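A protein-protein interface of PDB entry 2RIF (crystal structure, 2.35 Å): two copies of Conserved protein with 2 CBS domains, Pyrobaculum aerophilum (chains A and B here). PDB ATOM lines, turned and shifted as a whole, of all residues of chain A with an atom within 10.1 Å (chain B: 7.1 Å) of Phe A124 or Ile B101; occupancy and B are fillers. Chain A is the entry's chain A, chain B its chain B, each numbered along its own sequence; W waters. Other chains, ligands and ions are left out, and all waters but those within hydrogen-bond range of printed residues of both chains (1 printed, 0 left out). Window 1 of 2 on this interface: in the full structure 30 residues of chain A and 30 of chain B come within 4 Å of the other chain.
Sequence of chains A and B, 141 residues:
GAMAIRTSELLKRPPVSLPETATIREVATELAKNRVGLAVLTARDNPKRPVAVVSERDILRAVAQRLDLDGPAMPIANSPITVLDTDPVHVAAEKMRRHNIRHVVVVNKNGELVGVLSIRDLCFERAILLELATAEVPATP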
ATOM      1  N   LEU A  10      20.488  12.336   0.172  1.00  0.00           N
ATOM      2  CA  LEU A  10      19.950  10.976   0.288  1.00  0.00           C
ATOM      3  C   LEU A  10      20.576  10.187   1.445  1.00  0.00           C
ATOM      4  O   LEU A  10      20.216   9.033   1.668  1.00  0.00           O
ATOM      5  CB  LEU A  10      20.132  10.203  -1.024  1.00  0.00           C
ATOM      6  CG  LEU A  10      19.378  10.727  -2.248  1.00  0.00           C
ATOM      7  CD1 LEU A  10      19.657   9.843  -3.452  1.00  0.00           C
ATOM      8  CD2 LEU A  10      17.881  10.806  -1.983  1.00  0.00           C
ATOM      9  N   LYS A  12      20.862   9.146   5.183  1.00  0.00           N
ATOM     10  CA  LYS A  12      19.960   9.099   6.341  1.00  0.00           C
ATOM     11  C   LYS A  12      20.547   8.369   7.558  1.00  0.00           C
ATOM     12  O   LYS A  12      19.845   8.165   8.551  1.00  0.00           O
ATOM     13  CB  LYS A  12      18.623   8.450   5.948  1.00  0.00           C
ATOM     14  CG  LYS A  12      18.737   7.055   5.317  1.00  0.00           C
ATOM     15  CD  LYS A  12      18.722   7.104   3.794  1.00  0.00           C
ATOM     16  CE  LYS A  12      17.314   7.328   3.246  1.00  0.00           C
ATOM     17  NZ  LYS A  12      17.276   7.283   1.758  1.00  0.00           N
ATOM     18  N   VAL A  89      23.159  12.812  -7.660  1.00  0.00           N
ATOM     19  CA  VAL A  89      22.845  11.405  -7.386  1.00  0.00           C
ATOM     20  C   VAL A  89      23.029  10.478  -8.595  1.00  0.00           C
ATOM     21  O   VAL A  89      23.386   9.309  -8.432  1.00  0.00           O
ATOM     22  CB  VAL A  89      21.404  11.254  -6.841  1.00  0.00           C
ATOM     23  CG1 VAL A  89      21.070   9.791  -6.583  1.00  0.00           C
ATOM     24  CG2 VAL A  89      21.230  12.067  -5.566  1.00  0.00           C
ATOM     25  N   ARG A 102      26.228  -2.469  -5.822  1.00  0.00           N
ATOM     26  CA  ARG A 102      24.984  -1.945  -5.265  1.00  0.00           C
ATOM     27  C   ARG A 102      25.244  -0.946  -4.137  1.00  0.00           C
ATOM     28  O   ARG A 102      24.334  -0.614  -3.372  1.00  0.00           O
ATOM     29  CB  ARG A 102      24.111  -3.099  -4.772  1.00  0.00           C
ATOM     30  CG  ARG A 102      23.690  -4.066  -5.885  1.00  0.00           C
ATOM     31  CD  ARG A 102      22.954  -5.300  -5.362  1.00  0.00           C
ATOM     32  NE  ARG A 102      23.802  -6.111  -4.490  1.00  0.00           N
ATOM     33  CZ  ARG A 102      23.472  -7.305  -4.004  1.00  0.00           C
ATOM     34  NH1 ARG A 102      22.297  -7.863  -4.283  1.00  0.00           N
ATOM     35  NH2 ARG A 102      24.331  -7.942  -3.218  1.00  0.00           N
ATOM     36  N   SER A 118      23.300   3.386  -1.262  1.00  0.00           N
ATOM     37  CA  SER A 118      22.952   2.053  -1.752  1.00  0.00           C
ATOM     38  C   SER A 118      21.988   2.133  -2.929  1.00  0.00           C
ATOM     39  O   SER A 118      21.267   3.116  -3.088  1.00  0.00           O
ATOM     40  CB  SER A 118      22.317   1.239  -0.618  1.00  0.00           C
ATOM     41  OG  SER A 118      21.637   0.094  -1.101  1.00  0.00           O
ATOM     42  N   ILE A 119      21.973   1.080  -3.745  1.00  0.00           N
ATOM     43  CA  ILE A 119      21.015   0.961  -4.849  1.00  0.00           C
ATOM     44  C   ILE A 119      19.569   1.012  -4.328  1.00  0.00           C
ATOM     45  O   ILE A 119      18.647   1.378  -5.054  1.00  0.00           O
ATOM     46  CB  ILE A 119      21.247  -0.347  -5.649  1.00  0.00           C
ATOM     47  CG1 ILE A 119      20.509  -0.308  -6.988  1.00  0.00           C
ATOM     48  CG2 ILE A 119      20.816  -1.564  -4.836  1.00  0.00           C
ATOM     49  CD1 ILE A 119      20.890  -1.438  -7.916  1.00  0.00           C
ATOM     50  N   ARG A 120      19.390   0.637  -3.064  1.00  0.00           N
ATOM     51  CA  ARG A 120      18.098   0.708  -2.386  1.00  0.00           C
ATOM     52  C   ARG A 120      17.605   2.158  -2.258  1.00  0.00           C
ATOM     53  O   ARG A 120      16.404   2.421  -2.334  1.00  0.00           O
ATOM     54  CB  ARG A 120      18.222   0.066  -0.998  1.00  0.00           C
ATOM     55  CG  ARG A 120      16.952  -0.550  -0.461  1.00  0.00           C
ATOM     56  CD  ARG A 120      17.165  -1.100   0.942  1.00  0.00           C
ATOM     57  NE  ARG A 120      18.114  -2.215   0.969  1.00  0.00           N
ATOM     58  CZ  ARG A 120      17.808  -3.501   0.789  1.00  0.00           C
ATOM     59  NH1 ARG A 120      16.558  -3.892   0.554  1.00  0.00           N
ATOM     60  NH2 ARG A 120      18.771  -4.416   0.843  1.00  0.00           N
ATOM     61  N   ASP A 121      18.541   3.091  -2.071  1.00  0.00           N
ATOM     62  CA  ASP A 121      18.220   4.517  -1.923  1.00  0.00           C
ATOM     63  C   ASP A 121      17.748   5.165  -3.224  1.00  0.00           C
ATOM     64  O   ASP A 121      16.874   6.033  -3.208  1.00  0.00           O
ATOM     65  CB  ASP A 121      19.442   5.299  -1.425  1.00  0.00           C
ATOM     66  CG  ASP A 121      19.941   4.819  -0.079  1.00  0.00           C
ATOM     67  OD1 ASP A 121      19.106   4.556   0.813  1.00  0.00           O
ATOM     68  OD2 ASP A 121      21.176   4.718   0.088  1.00  0.00           O
ATOM     69  N   LEU A 122      18.337   4.746  -4.341  1.00  0.00           N
ATOM     70  CA  LEU A 122      18.085   5.373  -5.637  1.00  0.00           C
ATOM     71  C   LEU A 122      16.833   4.842  -6.331  1.00  0.00           C
ATOM     72  O   LEU A 122      16.173   5.575  -7.070  1.00  0.00           O
ATOM     73  CB  LEU A 122      19.289   5.164  -6.565  1.00  0.00           C
ATOM     74  CG  LEU A 122      20.678   5.446  -5.987  1.00  0.00           C
ATOM     75  CD1 LEU A 122      21.730   5.356  -7.083  1.00  0.00           C
ATOM     76  CD2 LEU A 122      20.726   6.808  -5.310  1.00  0.00           C
ATOM     77  N   CYS A 123      16.505   3.577  -6.083  1.00  0.00           N
ATOM     78  CA  CYS A 123      15.457   2.885  -6.832  1.00  0.00           C
ATOM     79  C   CYS A 123      14.062   2.930  -6.208  1.00  0.00           C
ATOM     80  O   CYS A 123      13.069   2.795  -6.925  1.00  0.00           O
ATOM     81  CB  CYS A 123      15.871   1.431  -7.041  1.00  0.00           C
ATOM     82  SG  CYS A 123      17.367   1.271  -8.026  1.00  0.00           S
ATOM     83  N   PHE A 124      13.984   3.125  -4.892  1.00  0.00           N
ATOM     84  CA  PHE A 124      12.697   3.084  -4.188  1.00  0.00           C
ATOM     85  C   PHE A 124      12.143   4.462  -3.802  1.00  0.00           C
ATOM     86  O   PHE A 124      11.557   4.621  -2.723  1.00  0.00           O
ATOM     87  CB  PHE A 124      12.791   2.186  -2.945  1.00  0.00           C
ATOM     88  CG  PHE A 124      13.241   0.770  -3.230  1.00  0.00           C
ATOM     89  CD1 PHE A 124      12.986   0.153  -4.456  1.00  0.00           C
ATOM     90  CD2 PHE A 124      13.886   0.036  -2.244  1.00  0.00           C
ATOM     91  CE1 PHE A 124      13.393  -1.153  -4.694  1.00  0.00           C
ATOM     92  CE2 PHE A 124      14.291  -1.273  -2.478  1.00  0.00           C
ATOM     93  CZ  PHE A 124      14.045  -1.866  -3.703  1.00  0.00           C
ATOM     94  N   GLU A 125      12.329   5.450  -4.681  1.00  0.00           N
ATOM     95  CA  GLU A 125      11.657   6.742  -4.538  1.00  0.00           C
ATOM     96  C   GLU A 125      11.393   7.341  -5.919  1.00  0.00           C
ATOM     97  O   GLU A 125      12.320   7.514  -6.713  1.00  0.00           O
ATOM     98  CB  GLU A 125      12.464   7.707  -3.664  1.00  0.00           C
ATOM     99  CG  GLU A 125      11.759   9.051  -3.433  1.00  0.00           C
ATOM    100  CD  GLU A 125      12.041   9.658  -2.064  1.00  0.00           C
ATOM    101  OE1 GLU A 125      13.156   9.464  -1.530  1.00  0.00           O
ATOM    102  OE2 GLU A 125      11.141  10.339  -1.523  1.00  0.00           O
ATOM    103  N   ARG A 126      10.124   7.643  -6.194  1.00  0.00           N
ATOM    104  CA  ARG A 126       9.703   8.169  -7.499  1.00  0.00           C
ATOM    105  C   ARG A 126      10.437   9.449  -7.901  1.00  0.00           C
ATOM    106  O   ARG A 126      10.717   9.659  -9.083  1.00  0.00           O
ATOM    107  CB  ARG A 126       8.187   8.424  -7.525  1.00  0.00           C
ATOM    108  CG  ARG A 126       7.331   7.193  -7.817  1.00  0.00           C
ATOM    109  CD  ARG A 126       7.122   6.313  -6.592  1.00  0.00           C
ATOM    110  NE  ARG A 126       6.089   5.301  -6.825  1.00  0.00           N
ATOM    111  CZ  ARG A 126       4.775   5.534  -6.829  1.00  0.00           C
ATOM    112  NH1 ARG A 126       4.293   6.757  -6.618  1.00  0.00           N
ATOM    113  NH2 ARG A 126       3.929   4.532  -7.052  1.00  0.00           N
ATOM    114  N   ALA A 127      10.738  10.299  -6.920  1.00  0.00           N
ATOM    115  CA  ALA A 127      11.441  11.559  -7.169  1.00  0.00           C
ATOM    116  C   ALA A 127      12.827  11.336  -7.779  1.00  0.00           C
ATOM    117  O   ALA A 127      13.258  12.099  -8.645  1.00  0.00           O
ATOM    118  CB  ALA A 127      11.558  12.361  -5.878  1.00  0.00           C
ATOM    119  N   ILE A 128      13.510  10.288  -7.326  1.00  0.00           N
ATOM    120  CA  ILE A 128      14.853   9.963  -7.805  1.00  0.00           C
ATOM    121  C   ILE A 128      14.801   9.247  -9.154  1.00  0.00           C
ATOM    122  O   ILE A 128      15.504   9.631 -10.091  1.00  0.00           O
ATOM    123  CB  ILE A 128      15.616   9.079  -6.793  1.00  0.00           C
ATOM    124  CG1 ILE A 128      15.767   9.804  -5.454  1.00  0.00           C
ATOM    125  CG2 ILE A 128      16.989   8.707  -7.337  1.00  0.00           C
ATOM    126  CD1 ILE A 128      16.429   8.968  -4.384  1.00  0.00           C
ATOM    127  N   LEU A 129      13.969   8.209  -9.243  1.00  0.00           N
ATOM    128  CA  LEU A 129      13.811   7.422 -10.473  1.00  0.00           C
ATOM    129  C   LEU A 129      13.601   8.299 -11.706  1.00  0.00           C
ATOM    130  O   LEU A 129      14.190   8.048 -12.760  1.00  0.00           O
ATOM    131  CB  LEU A 129      12.640   6.442 -10.337  1.00  0.00           C
ATOM    132  CG  LEU A 129      12.840   5.265  -9.380  1.00  0.00           C
ATOM    133  CD1 LEU A 129      11.528   4.527  -9.156  1.00  0.00           C
ATOM    134  CD2 LEU A 129      13.905   4.317  -9.906  1.00  0.00           C
ATOM    135  N   LEU A 130      12.760   9.321 -11.566  1.00  0.00           N
ATOM    136  CA  LEU A 130      12.492  10.268 -12.648  1.00  0.00           C
ATOM    137  C   LEU A 130      13.759  11.023 -13.058  1.00  0.00           C
ATOM    138  O   LEU A 130      14.007  11.225 -14.248  1.00  0.00           O
ATOM    139  CB  LEU A 130      11.399  11.259 -12.228  1.00  0.00           C
ATOM    140  CG  LEU A 130      10.982  12.341 -13.232  1.00  0.00           C
ATOM    141  CD1 LEU A 130      10.543  11.727 -14.553  1.00  0.00           C
ATOM    142  CD2 LEU A 130       9.873  13.204 -12.647  1.00  0.00           C
ATOM    143  N   LEU A 132      16.874   9.983 -12.589  1.00  0.00           N
ATOM    144  CA  LEU A 132      17.784   9.016 -13.204  1.00  0.00           C
ATOM    145  C   LEU A 132      17.428   8.811 -14.679  1.00  0.00           C
ATOM    146  O   LEU A 132      18.295   8.488 -15.493  1.00  0.00           O
ATOM    147  CB  LEU A 132      17.745   7.679 -12.456  1.00  0.00           C
ATOM    148  CG  LEU A 132      18.218   7.706 -10.998  1.00  0.00           C
ATOM    149  CD1 LEU A 132      18.052   6.335 -10.359  1.00  0.00           C
ATOM    150  CD2 LEU A 132      19.666   8.173 -10.903  1.00  0.00           C
ATOM    151  N   ILE B  81       8.216 -14.610  -2.797  1.00  0.00           N
ATOM    152  CA  ILE B  81       7.391 -13.515  -3.301  1.00  0.00           C
ATOM    153  C   ILE B  81       7.547 -13.535  -4.814  1.00  0.00           C
ATOM    154  O   ILE B  81       8.662 -13.424  -5.324  1.00  0.00           O
ATOM    155  CB  ILE B  81       7.849 -12.149  -2.757  1.00  0.00           C
ATOM    156  CG1 ILE B  81       7.670 -12.084  -1.235  1.00  0.00           C
ATOM    157  CG2 ILE B  81       7.078 -11.020  -3.425  1.00  0.00           C
ATOM    158  CD1 ILE B  81       6.237 -12.225  -0.775  1.00  0.00           C
ATOM    159  N   THR B  82       6.439 -13.671  -5.536  1.00  0.00           N
ATOM    160  CA  THR B  82       6.506 -13.931  -6.970  1.00  0.00           C
ATOM    161  C   THR B  82       5.824 -12.884  -7.850  1.00  0.00           C
ATOM    162  O   THR B  82       5.022 -12.077  -7.379  1.00  0.00           O
ATOM    163  CB  THR B  82       5.888 -15.313  -7.296  1.00  0.00           C
ATOM    164  OG1 THR B  82       4.500 -15.320  -6.941  1.00  0.00           O
ATOM    165  CG2 THR B  82       6.608 -16.423  -6.534  1.00  0.00           C
ATOM    166  N   ALA B  92       6.993  -5.952 -10.555  1.00  0.00           N
ATOM    167  CA  ALA B  92       8.179  -6.532  -9.935  1.00  0.00           C
ATOM    168  C   ALA B  92       8.959  -5.464  -9.169  1.00  0.00           C
ATOM    169  O   ALA B  92       9.490  -5.731  -8.092  1.00  0.00           O
ATOM    170  CB  ALA B  92       9.063  -7.181 -10.992  1.00  0.00           C
ATOM    171  N   ALA B  93       9.009  -4.255  -9.724  1.00  0.00           N
ATOM    172  CA  ALA B  93       9.738  -3.144  -9.112  1.00  0.00           C
ATOM    173  C   ALA B  93       9.117  -2.669  -7.799  1.00  0.00           C
ATOM    174  O   ALA B  93       9.838  -2.389  -6.840  1.00  0.00           O
ATOM    175  CB  ALA B  93       9.845  -1.978 -10.090  1.00  0.00           C
ATOM    176  N   GLU B  94       7.791  -2.570  -7.750  1.00  0.00           N
ATOM    177  CA  GLU B  94       7.132  -2.058  -6.549  1.00  0.00           C
ATOM    178  C   GLU B  94       7.033  -3.123  -5.452  1.00  0.00           C
ATOM    179  O   GLU B  94       6.967  -2.780  -4.273  1.00  0.00           O
ATOM    180  CB  GLU B  94       5.772  -1.421  -6.879  1.00  0.00           C
ATOM    181  CG  GLU B  94       4.567  -2.339  -6.867  1.00  0.00           C
ATOM    182  CD  GLU B  94       4.020  -2.614  -5.481  1.00  0.00           C
ATOM    183  OE1 GLU B  94       3.577  -3.755  -5.253  1.00  0.00           O
ATOM    184  OE2 GLU B  94       4.029  -1.701  -4.625  1.00  0.00           O
ATOM    185  N   LYS B  95       7.030  -4.401  -5.834  1.00  0.00           N
ATOM    186  CA  LYS B  95       7.082  -5.491  -4.852  1.00  0.00           C
ATOM    187  C   LYS B  95       8.426  -5.484  -4.123  1.00  0.00           C
ATOM    188  O   LYS B  95       8.483  -5.729  -2.919  1.00  0.00           O
ATOM    189  CB  LYS B  95       6.831  -6.859  -5.507  1.00  0.00           C
ATOM    190  CG  LYS B  95       5.357  -7.150  -5.763  1.00  0.00           C
ATOM    191  CD  LYS B  95       5.104  -8.610  -6.107  1.00  0.00           C
ATOM    192  CE  LYS B  95       3.609  -8.903  -6.151  1.00  0.00           C
ATOM    193  NZ  LYS B  95       3.300 -10.334  -6.421  1.00  0.00           N
ATOM    194  N   MET B  96       9.498  -5.197  -4.861  1.00  0.00           N
ATOM    195  CA  MET B  96      10.834  -5.046  -4.280  1.00  0.00           C
ATOM    196  C   MET B  96      10.877  -3.884  -3.287  1.00  0.00           C
ATOM    197  O   MET B  96      11.425  -4.013  -2.191  1.00  0.00           O
ATOM    198  CB  MET B  96      11.876  -4.822  -5.379  1.00  0.00           C
ATOM    199  CG  MET B  96      12.238  -6.073  -6.157  1.00  0.00           C
ATOM    200  SD  MET B  96      13.431  -5.724  -7.460  1.00  0.00           S
ATOM    201  CE  MET B  96      13.394  -7.256  -8.389  1.00  0.00           C
ATOM    202  N   ARG B  97      10.305  -2.752  -3.694  1.00  0.00           N
ATOM    203  CA  ARG B  97      10.201  -1.570  -2.839  1.00  0.00           C
ATOM    204  C   ARG B  97       9.312  -1.835  -1.620  1.00  0.00           C
ATOM    205  O   ARG B  97       9.641  -1.425  -0.505  1.00  0.00           O
ATOM    206  CB  ARG B  97       9.653  -0.385  -3.649  1.00  0.00           C
ATOM    207  CG  ARG B  97       9.191   0.809  -2.821  1.00  0.00           C
ATOM    208  CD  ARG B  97       9.094   2.091  -3.648  1.00  0.00           C
ATOM    209  NE  ARG B  97       8.656   1.875  -5.032  1.00  0.00           N
ATOM    210  CZ  ARG B  97       7.396   1.668  -5.419  1.00  0.00           C
ATOM    211  NH1 ARG B  97       6.402   1.619  -4.534  1.00  0.00           N
ATOM    212  NH2 ARG B  97       7.128   1.495  -6.710  1.00  0.00           N
ATOM    213  N   ARG B  98       8.197  -2.526  -1.845  1.00  0.00           N
ATOM    214  CA  ARG B  98       7.223  -2.808  -0.791  1.00  0.00           C
ATOM    215  C   ARG B  98       7.773  -3.773   0.263  1.00  0.00           C
ATOM    216  O   ARG B  98       7.717  -3.489   1.462  1.00  0.00           O
ATOM    217  CB  ARG B  98       5.920  -3.349  -1.396  1.00  0.00           C
ATOM    218  CG  ARG B  98       4.868  -3.752  -0.372  1.00  0.00           C
ATOM    219  CD  ARG B  98       3.448  -3.572  -0.893  1.00  0.00           C
ATOM    220  NE  ARG B  98       3.200  -4.201  -2.193  1.00  0.00           N
ATOM    221  CZ  ARG B  98       2.865  -5.480  -2.376  1.00  0.00           C
ATOM    222  NH1 ARG B  98       2.733  -6.314  -1.349  1.00  0.00           N
ATOM    223  NH2 ARG B  98       2.658  -5.941  -3.602  1.00  0.00           N
ATOM    224  N   HIS B  99       8.316  -4.900  -0.192  1.00  0.00           N
ATOM    225  CA  HIS B  99       8.845  -5.931   0.707  1.00  0.00           C
ATOM    226  C   HIS B  99      10.295  -5.687   1.136  1.00  0.00           C
ATOM    227  O   HIS B  99      10.841  -6.452   1.939  1.00  0.00           O
ATOM    228  CB  HIS B  99       8.726  -7.307   0.049  1.00  0.00           C
ATOM    229  CG  HIS B  99       7.313  -7.741  -0.183  1.00  0.00           C
ATOM    230  ND1 HIS B  99       6.708  -7.681  -1.419  1.00  0.00           N
ATOM    231  CD2 HIS B  99       6.383  -8.231   0.670  1.00  0.00           C
ATOM    232  CE1 HIS B  99       5.466  -8.122  -1.320  1.00  0.00           C
ATOM    233  NE2 HIS B  99       5.243  -8.461  -0.063  1.00  0.00           N
ATOM    234  N   ASN B 100      10.907  -4.624   0.613  1.00  0.00           N
ATOM    235  CA  ASN B 100      12.305  -4.301   0.887  1.00  0.00           C
ATOM    236  C   ASN B 100      13.216  -5.475   0.506  1.00  0.00           C
ATOM    237  O   ASN B 100      14.113  -5.862   1.257  1.00  0.00           O
ATOM    238  CB  ASN B 100      12.489  -3.885   2.355  1.00  0.00           C
ATOM    239  CG  ASN B 100      13.742  -3.049   2.578  1.00  0.00           C
ATOM    240  OD1 ASN B 100      14.031  -2.125   1.815  1.00  0.00           O
ATOM    241  ND2 ASN B 100      14.484  -3.359   3.638  1.00  0.00           N
ATOM    242  N   ILE B 101      12.948  -6.046  -0.669  1.00  0.00           N
ATOM    243  CA  ILE B 101      13.747  -7.134  -1.234  1.00  0.00           C
ATOM    244  C   ILE B 101      14.372  -6.648  -2.535  1.00  0.00           C
ATOM    245  O   ILE B 101      13.875  -5.708  -3.154  1.00  0.00           O
ATOM    246  CB  ILE B 101      12.912  -8.425  -1.501  1.00  0.00           C
ATOM    247  CG1 ILE B 101      11.731  -8.164  -2.442  1.00  0.00           C
ATOM    248  CG2 ILE B 101      12.393  -9.009  -0.205  1.00  0.00           C
ATOM    249  CD1 ILE B 101      10.811  -9.358  -2.598  1.00  0.00           C
ATOM    250  N   ARG B 102      15.466  -7.283  -2.938  1.00  0.00           N
ATOM    251  CA  ARG B 102      16.161  -6.915  -4.169  1.00  0.00           C
ATOM    252  C   ARG B 102      16.023  -7.997  -5.236  1.00  0.00           C
ATOM    253  O   ARG B 102      16.734  -7.982  -6.238  1.00  0.00           O
ATOM    254  CB  ARG B 102      17.628  -6.630  -3.870  1.00  0.00           C
ATOM    255  CG  ARG B 102      17.832  -5.422  -2.962  1.00  0.00           C
ATOM    256  CD  ARG B 102      19.280  -5.273  -2.535  1.00  0.00           C
ATOM    257  NE  ARG B 102      19.698  -6.367  -1.662  1.00  0.00           N
ATOM    258  CZ  ARG B 102      20.907  -6.489  -1.124  1.00  0.00           C
ATOM    259  NH1 ARG B 102      21.848  -5.583  -1.363  1.00  0.00           N
ATOM    260  NH2 ARG B 102      21.170  -7.531  -0.345  1.00  0.00           N
ATOM    261  N   HIS B 103      15.096  -8.927  -5.013  1.00  0.00           N
ATOM    262  CA  HIS B 103      14.789  -9.980  -5.974  1.00  0.00           C
ATOM    263  C   HIS B 103      13.303 -10.288  -5.971  1.00  0.00           C
ATOM    264  O   HIS B 103      12.628 -10.127  -4.955  1.00  0.00           O
ATOM    265  CB  HIS B 103      15.542 -11.266  -5.633  1.00  0.00           C
ATOM    266  CG  HIS B 103      17.028 -11.138  -5.721  1.00  0.00           C
ATOM    267  ND1 HIS B 103      17.788 -10.606  -4.703  1.00  0.00           N
ATOM    268  CD2 HIS B 103      17.896 -11.477  -6.703  1.00  0.00           C
ATOM    269  CE1 HIS B 103      19.061 -10.621  -5.054  1.00  0.00           C
ATOM    270  NE2 HIS B 103      19.154 -11.143  -6.263  1.00  0.00           N
ATOM    271  N   VAL B 104      12.804 -10.724  -7.122  1.00  0.00           N
ATOM    272  CA  VAL B 104      11.461 -11.281  -7.238  1.00  0.00           C
ATOM    273  C   VAL B 104      11.561 -12.519  -8.121  1.00  0.00           C
ATOM    274  O   VAL B 104      12.251 -12.505  -9.145  1.00  0.00           O
ATOM    275  CB  VAL B 104      10.445 -10.275  -7.834  1.00  0.00           C
ATOM    276  CG1 VAL B 104      10.161  -9.161  -6.848  1.00  0.00           C
ATOM    277  CG2 VAL B 104      10.946  -9.709  -9.154  1.00  0.00           C
ATOM    278  N   VAL B 105      10.896 -13.592  -7.705  1.00  0.00           N
ATOM    279  CA  VAL B 105      10.911 -14.846  -8.450  1.00  0.00           C
ATOM    280  C   VAL B 105       9.824 -14.791  -9.515  1.00  0.00           C
ATOM    281  O   VAL B 105       8.655 -14.559  -9.203  1.00  0.00           O
ATOM    282  CB  VAL B 105      10.662 -16.054  -7.529  1.00  0.00           C
ATOM    283  CG1 VAL B 105      10.748 -17.351  -8.321  1.00  0.00           C
ATOM    284  CG2 VAL B 105      11.658 -16.061  -6.371  1.00  0.00           C
ATOM    285  N   ILE B 119      16.756  -6.247  -8.598  1.00  0.00           N
ATOM    286  CA  ILE B 119      16.714  -4.779  -8.612  1.00  0.00           C
ATOM    287  C   ILE B 119      17.742  -4.236  -9.615  1.00  0.00           C
ATOM    288  O   ILE B 119      17.532  -3.194 -10.238  1.00  0.00           O
ATOM    289  CB  ILE B 119      16.980  -4.190  -7.200  1.00  0.00           C
ATOM    290  CG1 ILE B 119      16.710  -2.684  -7.175  1.00  0.00           C
ATOM    291  CG2 ILE B 119      18.407  -4.482  -6.742  1.00  0.00           C
ATOM    292  CD1 ILE B 119      16.832  -2.074  -5.795  1.00  0.00           C
ATOM    293  N   CYS B 123      16.921  -1.001 -12.489  1.00  0.00           N
ATOM    294  CA  CYS B 123      17.469   0.337 -12.254  1.00  0.00           C
ATOM    295  C   CYS B 123      18.542   0.787 -13.244  1.00  0.00           C
ATOM    296  O   CYS B 123      18.710   1.988 -13.465  1.00  0.00           O
ATOM    297  CB  CYS B 123      18.025   0.416 -10.833  1.00  0.00           C
ATOM    298  SG  CYS B 123      16.761   0.139  -9.593  1.00  0.00           S
HETATM  299  O   HOH W   1      21.950  -2.601  -1.595  1.00  0.00           O
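Among the printed residues, pairs that only touch across the chains: Phe A124 with Arg B97 (3.5 Å), Phe A124 with Ile B119 (3.5 Å), Arg A102 with Arg B102 (3.5 Å), Phe A124 with Met B96 (3.7 Å), Cys A123 with Ile B119 (3.8 Å), Phe A124 with Ile B101 (3.9 Å), Arg A126 with Arg B97 (3.9 Å) and Ile A119 with Ile B119 (3.97 Å).
Water W1 bridges OG of Ser A118 (2.8 Å) and NH1 of Arg B102 (3.0 Å).
The guanidinium group (NE) of Arg B102 lies close to the guanidinium group (NH2) of Arg A120.
The side-chain sulfur of Cys A123 is disulfide-bonded to the side-chain sulfur of Cys B123.
The backbone carbonyl oxygen (O) of Asn B100 lies within hydrogen-bond range of the guanidinium group (NH1) of Arg A120 (3.2 Å).
Arg B102 touches its own counterpart, Arg A102.
Ile A119 touches its own counterpart, Ile B119.
Cys A123 touches Ile B119, but with the chains exchanged Ile A119 does not touch Cys B123 (4.5 Å).
Cys A123 touches its own counterpart, Cys B123.
Positions printed for both chains: 102, 119 and 123.
Of the 11 pairs that touch across the chains among the printed residues, 3 have their exchanged pair printed and touching as well.
Hydrophobic or aromatic side chains of chain A that line the printed part of chain B: Phe A124.
Along chain A the printed residues that touch a printed residue of chain B span positions 102 to 126.
Of the 18 printed residues of chain B, 7 touch a printed residue of chain A.
Printed residues of chain B that touch a printed residue of chain A: Met B96, Arg B97, Asn B100, Ile B101, Arg B102, Ile B119 and Cys B123.
Among the printed residues, 11 pairs touch across the chains.
Among the printed residues, no Asp or Glu carboxylate lies within 4 Å of a Lys or Arg side-chain nitrogen of the other chain.
Of the printed residues of chain B, Phe A124 touches Met B96 (3.7 Å), Arg B97 (3.5 Å), Ile B101 (3.9 Å) and Ile B119 (3.5 Å).
Ile B101 touches just one residue of chain A: Phe A124 (3.9 Å).
No residue of chain A comes within 4 Å of Ile B81.
Printed residues of chain B within 4 Å of Arg A126: Arg B97.
Printed residues of chain B within 4 Å of Arg A102: Arg B102 (3.5 Å).
Of the printed residues of chain A, Arg B102 touches Arg A102 and Arg A120.
Ala B92 touches none of the printed residues of chain A.
The nearest printed residue of chain A that does not touch Arg B97 is Glu A125 (4.8 Å).
N of Arg A120 sits close to OG of Ser A118, at 3.0 Å.
N of Ile B119 sits close to SD of Met B96, 3.6 Å away.
O of Arg B102 sits at hydrogen-bond distance from N of Ile B119 (2.9 Å).
N of Ile A119 sits at hydrogen-bond distance from O of Arg A102 (2.9 Å).
The backbone NH of Ile B101 is in hydrogen-bond range of the backbone carbonyl oxygen of Met B96 (3.0 Å).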
